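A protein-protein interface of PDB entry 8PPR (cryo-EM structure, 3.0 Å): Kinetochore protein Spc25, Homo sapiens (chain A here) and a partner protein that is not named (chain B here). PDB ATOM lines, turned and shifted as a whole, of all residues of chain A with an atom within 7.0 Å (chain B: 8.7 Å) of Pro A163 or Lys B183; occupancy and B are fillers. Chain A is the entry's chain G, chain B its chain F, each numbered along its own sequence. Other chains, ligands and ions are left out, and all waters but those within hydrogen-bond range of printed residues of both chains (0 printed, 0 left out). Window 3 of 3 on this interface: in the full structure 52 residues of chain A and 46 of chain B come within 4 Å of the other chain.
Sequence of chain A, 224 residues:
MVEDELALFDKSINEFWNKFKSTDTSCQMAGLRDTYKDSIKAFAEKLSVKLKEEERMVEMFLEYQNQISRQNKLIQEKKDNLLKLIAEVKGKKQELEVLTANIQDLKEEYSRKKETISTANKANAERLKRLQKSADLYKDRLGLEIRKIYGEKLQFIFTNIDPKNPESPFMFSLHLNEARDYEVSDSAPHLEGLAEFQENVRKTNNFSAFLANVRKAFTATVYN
NH2 of Arg B182 lies close to ND2 of Asn A160 (3.0 Å).
NZ of Lys B183 lies within hydrogen-bond range of O of Ile A161 (3.0 Å).
N of Pro A163 sits close to NZ of Lys B183 (3.4 Å).
The indole nitrogen (NE1) of Trp B190 lies close to the guanidinium group (NH1) of Arg A215.
OD1 of Asp B187 is in salt-bridge range of NE of Arg A215 (3.9 Å).
Among the printed residues, merely in contact across the chains: Asn A160 with Lys B183 (3.1 Å), Asn A160 with Ser B186 (3.5 Å), Asn A160 with Asp B187 (3.6 Å) and Asp A162 with Lys B183 (3.8 Å).
Pro A163 touches one residue of chain B.
Lys B183 touches four residues of chain A.
Printed residues of chain B within 4 Å of Arg A215: Asp B187 (2.4 Å) and Trp B190 (3.2 Å).
Of the printed residues of chain A, Ser B186 touches Asn A160 (3.5 Å).
Printed residues of chain B within 4 Å of Asn A160: Arg B182 (3.0 Å), Lys B183 (3.1 Å), Ser B186 (3.5 Å) and Asp B187 (3.6 Å).
Printed residues of chain B within 4 Å of Ile A161: Lys B183 (3.0 Å).
The backbone carbonyl oxygen (O) of Arg A215 is in hydrogen-bond range of the side-chain hydroxyl (OG1) of Thr A219, 3.1 Å away.
The side-chain carboxylate of Asp A162 is in salt-bridge range of the side-chain amino group of Lys A164 (2.8 Å).
The backbone carbonyl oxygen (O) of Pro A166 is in hydrogen-bond range of the backbone NH (N) of Asn A160 (2.5 Å).
OD2 of Asp A162 sits close to OD1 of Asn A165.
The backbone carbonyl oxygen of Asn A160 lies within hydrogen-bond range of the guanidinium group of Arg A215, at 3.1 Å.
The backbone carbonyl oxygen of Arg B182 lies within hydrogen-bond range of the side-chain hydroxyl of Ser B186 (3.1 Å).
Hydrophobic or aromatic side chains of chain B within 4 Å of the printed part of chain A: Trp B190.
Hydrophobic or aromatic side chains of chain A that line the printed part of chain B: Pro A163.
Among the printed residues, Asp or Glu carboxylates within 4 Å of a Lys or Arg side-chain nitrogen of the other chain: Arg A215 with Asp B187 (2.4 Å).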
ATOM      1  N   THR A 159     -29.756   3.040  -0.624  1.00  0.00           N
ATOM      2  CA  THR A 159     -28.930   3.333  -1.785  1.00  0.00           C
ATOM      3  C   THR A 159     -27.926   4.412  -1.415  1.00  0.00           C
ATOM      4  O   THR A 159     -27.864   4.829  -0.254  1.00  0.00           O
ATOM      5  CB  THR A 159     -29.788   3.774  -2.970  1.00  0.00           C
ATOM      6  OG1 THR A 159     -30.624   4.867  -2.572  1.00  0.00           O
ATOM      7  CG2 THR A 159     -30.662   2.625  -3.445  1.00  0.00           C
ATOM      8  N   ASN A 160     -27.147   4.877  -2.393  1.00  0.00           N
ATOM      9  CA  ASN A 160     -26.113   5.885  -2.158  1.00  0.00           C
ATOM     10  C   ASN A 160     -25.146   5.438  -1.066  1.00  0.00           C
ATOM     11  O   ASN A 160     -24.818   6.197  -0.153  1.00  0.00           O
ATOM     12  CB  ASN A 160     -26.728   7.243  -1.807  1.00  0.00           C
ATOM     13  CG  ASN A 160     -27.606   7.789  -2.911  1.00  0.00           C
ATOM     14  OD1 ASN A 160     -27.287   7.667  -4.092  1.00  0.00           O
ATOM     15  ND2 ASN A 160     -28.720   8.400  -2.530  1.00  0.00           N
ATOM     16  N   ILE A 161     -24.710   4.183  -1.138  1.00  0.00           N
ATOM     17  CA  ILE A 161     -23.733   3.630  -0.203  1.00  0.00           C
ATOM     18  C   ILE A 161     -22.454   3.220  -0.921  1.00  0.00           C
ATOM     19  O   ILE A 161     -21.364   3.685  -0.584  1.00  0.00           O
ATOM     20  CB  ILE A 161     -24.327   2.450   0.597  1.00  0.00           C
ATOM     21  CG1 ILE A 161     -25.509   2.913   1.443  1.00  0.00           C
ATOM     22  CG2 ILE A 161     -23.268   1.836   1.492  1.00  0.00           C
ATOM     23  CD1 ILE A 161     -26.254   1.774   2.087  1.00  0.00           C
ATOM     24  N   ASP A 162     -22.564   2.340  -1.905  1.00  0.00           N
ATOM     25  CA  ASP A 162     -21.390   1.888  -2.637  1.00  0.00           C
ATOM     26  C   ASP A 162     -20.901   3.014  -3.539  1.00  0.00           C
ATOM     27  O   ASP A 162     -21.652   3.463  -4.414  1.00  0.00           O
ATOM     28  CB  ASP A 162     -21.736   0.638  -3.442  1.00  0.00           C
ATOM     29  CG  ASP A 162     -20.519  -0.028  -4.053  1.00  0.00           C
ATOM     30  OD1 ASP A 162     -19.383   0.331  -3.683  1.00  0.00           O
ATOM     31  OD2 ASP A 162     -20.702  -0.943  -4.881  1.00  0.00           O
ATOM     32  N   PRO A 163     -19.676   3.513  -3.354  1.00  0.00           N
ATOM     33  CA  PRO A 163     -19.222   4.658  -4.162  1.00  0.00           C
ATOM     34  C   PRO A 163     -19.153   4.372  -5.650  1.00  0.00           C
ATOM     35  O   PRO A 163     -19.404   5.278  -6.455  1.00  0.00           O
ATOM     36  CB  PRO A 163     -17.834   4.979  -3.587  1.00  0.00           C
ATOM     37  CG  PRO A 163     -17.437   3.800  -2.775  1.00  0.00           C
ATOM     38  CD  PRO A 163     -18.672   3.067  -2.373  1.00  0.00           C
ATOM     39  N   LYS A 164     -18.815   3.142  -6.044  1.00  0.00           N
ATOM     40  CA  LYS A 164     -18.713   2.831  -7.467  1.00  0.00           C
ATOM     41  C   LYS A 164     -20.074   2.923  -8.149  1.00  0.00           C
ATOM     42  O   LYS A 164     -20.167   3.342  -9.308  1.00  0.00           O
ATOM     43  CB  LYS A 164     -18.083   1.451  -7.655  1.00  0.00           C
ATOM     44  CG  LYS A 164     -18.914   0.298  -7.131  1.00  0.00           C
ATOM     45  CD  LYS A 164     -18.218  -1.032  -7.341  1.00  0.00           C
ATOM     46  CE  LYS A 164     -17.069  -1.204  -6.361  1.00  0.00           C
ATOM     47  NZ  LYS A 164     -17.549  -1.302  -4.954  1.00  0.00           N
ATOM     48  N   ASN A 165     -21.138   2.540  -7.448  1.00  0.00           N
ATOM     49  CA  ASN A 165     -22.490   2.740  -7.949  1.00  0.00           C
ATOM     50  C   ASN A 165     -23.424   3.044  -6.785  1.00  0.00           C
ATOM     51  O   ASN A 165     -23.760   2.147  -6.000  1.00  0.00           O
ATOM     52  CB  ASN A 165     -22.978   1.517  -8.729  1.00  0.00           C
ATOM     53  CG  ASN A 165     -22.711   0.216  -8.005  1.00  0.00           C
ATOM     54  OD1 ASN A 165     -22.073   0.197  -6.955  1.00  0.00           O
ATOM     55  ND2 ASN A 165     -23.204  -0.883  -8.561  1.00  0.00           N
ATOM     56  N   PRO A 166     -23.861   4.297  -6.634  1.00  0.00           N
ATOM     57  CA  PRO A 166     -24.785   4.631  -5.541  1.00  0.00           C
ATOM     58  C   PRO A 166     -26.158   4.005  -5.696  1.00  0.00           C
ATOM     59  O   PRO A 166     -26.957   4.064  -4.754  1.00  0.00           O
ATOM     60  CB  PRO A 166     -24.867   6.162  -5.613  1.00  0.00           C
ATOM     61  CG  PRO A 166     -24.547   6.487  -7.031  1.00  0.00           C
ATOM     62  CD  PRO A 166     -23.548   5.462  -7.479  1.00  0.00           C
ATOM     63  N   PHE A 170     -29.215  -1.871  -1.074  1.00  0.00           N
ATOM     64  CA  PHE A 170     -28.879  -2.648   0.115  1.00  0.00           C
ATOM     65  C   PHE A 170     -30.160  -2.772   0.929  1.00  0.00           C
ATOM     66  O   PHE A 170     -30.515  -1.876   1.697  1.00  0.00           O
ATOM     67  CB  PHE A 170     -27.752  -1.989   0.901  1.00  0.00           C
ATOM     68  CG  PHE A 170     -26.510  -1.765   0.090  1.00  0.00           C
ATOM     69  CD1 PHE A 170     -26.377  -0.635  -0.700  1.00  0.00           C
ATOM     70  CD2 PHE A 170     -25.493  -2.703   0.087  1.00  0.00           C
ATOM     71  CE1 PHE A 170     -25.241  -0.433  -1.457  1.00  0.00           C
ATOM     72  CE2 PHE A 170     -24.357  -2.507  -0.672  1.00  0.00           C
ATOM     73  CZ  PHE A 170     -24.231  -1.369  -1.445  1.00  0.00           C
ATOM     74  N   ARG A 215     -27.207   1.175   8.324  1.00  0.00           N
ATOM     75  CA  ARG A 215     -26.471   1.822   7.244  1.00  0.00           C
ATOM     76  C   ARG A 215     -24.970   1.688   7.446  1.00  0.00           C
ATOM     77  O   ARG A 215     -24.224   1.478   6.484  1.00  0.00           O
ATOM     78  CB  ARG A 215     -26.861   3.296   7.146  1.00  0.00           C
ATOM     79  CG  ARG A 215     -26.408   3.963   5.859  1.00  0.00           C
ATOM     80  CD  ARG A 215     -26.272   5.464   6.045  1.00  0.00           C
ATOM     81  NE  ARG A 215     -25.573   6.111   4.939  1.00  0.00           N
ATOM     82  CZ  ARG A 215     -26.082   6.289   3.727  1.00  0.00           C
ATOM     83  NH1 ARG A 215     -27.305   5.889   3.423  1.00  0.00           N
ATOM     84  NH2 ARG A 215     -25.345   6.891   2.798  1.00  0.00           N
ATOM     85  N   THR A 219     -22.392  -0.111   4.939  1.00  0.00           N
ATOM     86  CA  THR A 219     -21.194   0.569   4.459  1.00  0.00           C
ATOM     87  C   THR A 219     -19.953  -0.277   4.705  1.00  0.00           C
ATOM     88  O   THR A 219     -19.082  -0.388   3.835  1.00  0.00           O
ATOM     89  CB  THR A 219     -21.063   1.932   5.138  1.00  0.00           C
ATOM     90  OG1 THR A 219     -22.095   2.805   4.662  1.00  0.00           O
ATOM     91  CG2 THR A 219     -19.708   2.554   4.836  1.00  0.00           C
ATOM     92  N   VAL A 222     -19.841  -3.060   2.211  1.00  0.00           N
ATOM     93  CA  VAL A 222     -19.469  -2.635   0.862  1.00  0.00           C
ATOM     94  C   VAL A 222     -17.969  -2.785   0.647  1.00  0.00           C
ATOM     95  O   VAL A 222     -17.517  -3.294  -0.386  1.00  0.00           O
ATOM     96  CB  VAL A 222     -19.923  -1.186   0.612  1.00  0.00           C
ATOM     97  CG1 VAL A 222     -19.338  -0.667  -0.686  1.00  0.00           C
ATOM     98  CG2 VAL A 222     -21.427  -1.109   0.573  1.00  0.00           C
ATOM     99  N   TYR A 223     -17.175  -2.349   1.623  1.00  0.00           N
ATOM    100  CA  TYR A 223     -15.728  -2.332   1.462  1.00  0.00           C
ATOM    101  C   TYR A 223     -15.106  -3.716   1.560  1.00  0.00           C
ATOM    102  O   TYR A 223     -13.899  -3.850   1.331  1.00  0.00           O
ATOM    103  CB  TYR A 223     -15.113  -1.399   2.502  1.00  0.00           C
ATOM    104  CG  TYR A 223     -15.573   0.029   2.341  1.00  0.00           C
ATOM    105  CD1 TYR A 223     -15.581   0.637   1.094  1.00  0.00           C
ATOM    106  CD2 TYR A 223     -16.018   0.761   3.432  1.00  0.00           C
ATOM    107  CE1 TYR A 223     -16.009   1.939   0.938  1.00  0.00           C
ATOM    108  CE2 TYR A 223     -16.448   2.065   3.287  1.00  0.00           C
ATOM    109  CZ  TYR A 223     -16.442   2.649   2.037  1.00  0.00           C
ATOM    110  OH  TYR A 223     -16.868   3.947   1.888  1.00  0.00           O
ATOM    111  N   SER B 177     -28.414  21.095  -3.299  1.00  0.00           N
ATOM    112  CA  SER B 177     -28.291  19.919  -4.150  1.00  0.00           C
ATOM    113  C   SER B 177     -27.693  20.237  -5.511  1.00  0.00           C
ATOM    114  O   SER B 177     -27.174  19.328  -6.168  1.00  0.00           O
ATOM    115  CB  SER B 177     -29.660  19.263  -4.334  1.00  0.00           C
ATOM    116  OG  SER B 177     -29.562  18.112  -5.154  1.00  0.00           O
ATOM    117  N   LEU B 180     -23.952  19.718  -4.676  1.00  0.00           N
ATOM    118  CA  LEU B 180     -23.562  18.552  -3.899  1.00  0.00           C
ATOM    119  C   LEU B 180     -24.213  17.304  -4.471  1.00  0.00           C
ATOM    120  O   LEU B 180     -25.382  17.327  -4.868  1.00  0.00           O
ATOM    121  CB  LEU B 180     -23.951  18.716  -2.430  1.00  0.00           C
ATOM    122  CG  LEU B 180     -23.411  19.985  -1.773  1.00  0.00           C
ATOM    123  CD1 LEU B 180     -24.113  20.248  -0.452  1.00  0.00           C
ATOM    124  CD2 LEU B 180     -21.905  19.893  -1.586  1.00  0.00           C
ATOM    125  N   SER B 181     -23.449  16.218  -4.510  1.00  0.00           N
ATOM    126  CA  SER B 181     -23.970  14.958  -5.007  1.00  0.00           C
ATOM    127  C   SER B 181     -24.955  14.359  -4.009  1.00  0.00           C
ATOM    128  O   SER B 181     -24.947  14.674  -2.816  1.00  0.00           O
ATOM    129  CB  SER B 181     -22.833  13.972  -5.269  1.00  0.00           C
ATOM    130  OG  SER B 181     -21.896  13.989  -4.206  1.00  0.00           O
ATOM    131  N   ARG B 182     -25.817  13.478  -4.520  1.00  0.00           N
ATOM    132  CA  ARG B 182     -26.749  12.771  -3.650  1.00  0.00           C
ATOM    133  C   ARG B 182     -26.004  11.890  -2.657  1.00  0.00           C
ATOM    134  O   ARG B 182     -26.429  11.743  -1.506  1.00  0.00           O
ATOM    135  CB  ARG B 182     -27.716  11.933  -4.483  1.00  0.00           C
ATOM    136  CG  ARG B 182     -28.677  12.747  -5.324  1.00  0.00           C
ATOM    137  CD  ARG B 182     -29.812  11.874  -5.824  1.00  0.00           C
ATOM    138  NE  ARG B 182     -30.376  11.064  -4.752  1.00  0.00           N
ATOM    139  CZ  ARG B 182     -30.760   9.802  -4.887  1.00  0.00           C
ATOM    140  NH1 ARG B 182     -30.636   9.161  -6.038  1.00  0.00           N
ATOM    141  NH2 ARG B 182     -31.282   9.167  -3.841  1.00  0.00           N
ATOM    142  N   LYS B 183     -24.897  11.288  -3.093  1.00  0.00           N
ATOM    143  CA  LYS B 183     -24.082  10.477  -2.197  1.00  0.00           C
ATOM    144  C   LYS B 183     -23.624  11.286  -0.992  1.00  0.00           C
ATOM    145  O   LYS B 183     -23.828  10.882   0.160  1.00  0.00           O
ATOM    146  CB  LYS B 183     -22.877   9.925  -2.959  1.00  0.00           C
ATOM    147  CG  LYS B 183     -21.977   9.023  -2.143  1.00  0.00           C
ATOM    148  CD  LYS B 183     -22.678   7.736  -1.780  1.00  0.00           C
ATOM    149  CE  LYS B 183     -21.782   6.839  -0.948  1.00  0.00           C
ATOM    150  NZ  LYS B 183     -20.609   6.354  -1.721  1.00  0.00           N
ATOM    151  N   PHE B 184     -23.020  12.449  -1.245  1.00  0.00           N
ATOM    152  CA  PHE B 184     -22.535  13.286  -0.155  1.00  0.00           C
ATOM    153  C   PHE B 184     -23.675  13.763   0.730  1.00  0.00           C
ATOM    154  O   PHE B 184     -23.548  13.785   1.959  1.00  0.00           O
ATOM    155  CB  PHE B 184     -21.771  14.485  -0.709  1.00  0.00           C
ATOM    156  CG  PHE B 184     -21.541  15.563   0.304  1.00  0.00           C
ATOM    157  CD1 PHE B 184     -20.612  15.393   1.315  1.00  0.00           C
ATOM    158  CD2 PHE B 184     -22.269  16.739   0.258  1.00  0.00           C
ATOM    159  CE1 PHE B 184     -20.404  16.381   2.256  1.00  0.00           C
ATOM    160  CE2 PHE B 184     -22.068  17.730   1.197  1.00  0.00           C
ATOM    161  CZ  PHE B 184     -21.133  17.552   2.196  1.00  0.00           C
ATOM    162  N   ILE B 185     -24.790  14.166   0.123  1.00  0.00           N
ATOM    163  CA  ILE B 185     -25.905  14.698   0.898  1.00  0.00           C
ATOM    164  C   ILE B 185     -26.459  13.630   1.829  1.00  0.00           C
ATOM    165  O   ILE B 185     -26.660  13.864   3.027  1.00  0.00           O
ATOM    166  CB  ILE B 185     -26.989  15.249  -0.045  1.00  0.00           C
ATOM    167  CG1 ILE B 185     -26.534  16.581  -0.646  1.00  0.00           C
ATOM    168  CG2 ILE B 185     -28.308  15.407   0.693  1.00  0.00           C
ATOM    169  CD1 ILE B 185     -27.606  17.298  -1.433  1.00  0.00           C
ATOM    170  N   SER B 186     -26.696  12.431   1.292  1.00  0.00           N
ATOM    171  CA  SER B 186     -27.218  11.344   2.112  1.00  0.00           C
ATOM    172  C   SER B 186     -26.232  10.958   3.205  1.00  0.00           C
ATOM    173  O   SER B 186     -26.629  10.725   4.353  1.00  0.00           O
ATOM    174  CB  SER B 186     -27.546  10.137   1.235  1.00  0.00           C
ATOM    175  OG  SER B 186     -28.572  10.446   0.308  1.00  0.00           O
ATOM    176  N   ASP B 187     -24.942  10.890   2.870  1.00  0.00           N
ATOM    177  CA  ASP B 187     -23.949  10.507   3.865  1.00  0.00           C
ATOM    178  C   ASP B 187     -23.868  11.533   4.988  1.00  0.00           C
ATOM    179  O   ASP B 187     -23.795  11.167   6.166  1.00  0.00           O
ATOM    180  CB  ASP B 187     -22.589  10.329   3.196  1.00  0.00           C
ATOM    181  CG  ASP B 187     -22.449   8.980   2.524  1.00  0.00           C
ATOM    182  OD1 ASP B 187     -23.462   8.255   2.434  1.00  0.00           O
ATOM    183  OD2 ASP B 187     -21.331   8.645   2.082  1.00  0.00           O
ATOM    184  N   TYR B 188     -23.889  12.821   4.645  1.00  0.00           N
ATOM    185  CA  TYR B 188     -23.861  13.863   5.663  1.00  0.00           C
ATOM    186  C   TYR B 188     -25.107  13.810   6.534  1.00  0.00           C
ATOM    187  O   TYR B 188     -25.023  13.927   7.762  1.00  0.00           O
ATOM    188  CB  TYR B 188     -23.728  15.234   5.005  1.00  0.00           C
ATOM    189  CG  TYR B 188     -24.276  16.357   5.851  1.00  0.00           C
ATOM    190  CD1 TYR B 188     -23.546  16.872   6.912  1.00  0.00           C
ATOM    191  CD2 TYR B 188     -25.526  16.898   5.590  1.00  0.00           C
ATOM    192  CE1 TYR B 188     -24.048  17.898   7.689  1.00  0.00           C
ATOM    193  CE2 TYR B 188     -26.035  17.923   6.360  1.00  0.00           C
ATOM    194  CZ  TYR B 188     -25.292  18.420   7.407  1.00  0.00           C
ATOM    195  OH  TYR B 188     -25.797  19.443   8.178  1.00  0.00           O
ATOM    196  N   LEU B 189     -26.277  13.642   5.914  1.00  0.00           N
ATOM    197  CA  LEU B 189     -27.513  13.600   6.683  1.00  0.00           C
ATOM    198  C   LEU B 189     -27.525  12.414   7.633  1.00  0.00           C
ATOM    199  O   LEU B 189     -27.978  12.527   8.778  1.00  0.00           O
ATOM    200  CB  LEU B 189     -28.711  13.547   5.741  1.00  0.00           C
ATOM    201  CG  LEU B 189     -29.005  14.863   5.023  1.00  0.00           C
ATOM    202  CD1 LEU B 189     -30.299  14.765   4.234  1.00  0.00           C
ATOM    203  CD2 LEU B 189     -29.060  16.010   6.018  1.00  0.00           C
ATOM    204  N   TRP B 190     -27.022  11.267   7.180  1.00  0.00           N
ATOM    205  CA  TRP B 190     -26.973  10.094   8.039  1.00  0.00           C
ATOM    206  C   TRP B 190     -25.905  10.221   9.112  1.00  0.00           C
ATOM    207  O   TRP B 190     -26.033   9.616  10.183  1.00  0.00           O
ATOM    208  CB  TRP B 190     -26.732   8.848   7.192  1.00  0.00           C
ATOM    209  CG  TRP B 190     -27.981   8.342   6.562  1.00  0.00           C
ATOM    210  CD1 TRP B 190     -28.271   8.306   5.231  1.00  0.00           C
ATOM    211  CD2 TRP B 190     -29.121   7.804   7.238  1.00  0.00           C
ATOM    212  NE1 TRP B 190     -29.522   7.775   5.035  1.00  0.00           N
ATOM    213  CE2 TRP B 190     -30.065   7.459   6.253  1.00  0.00           C
ATOM    214  CE3 TRP B 190     -29.436   7.577   8.581  1.00  0.00           C
ATOM    215  CZ2 TRP B 190     -31.301   6.900   6.566  1.00  0.00           C
ATOM    216  CZ3 TRP B 190     -30.662   7.023   8.892  1.00  0.00           C
ATOM    217  CH2 TRP B 190     -31.579   6.691   7.889  1.00  0.00           C
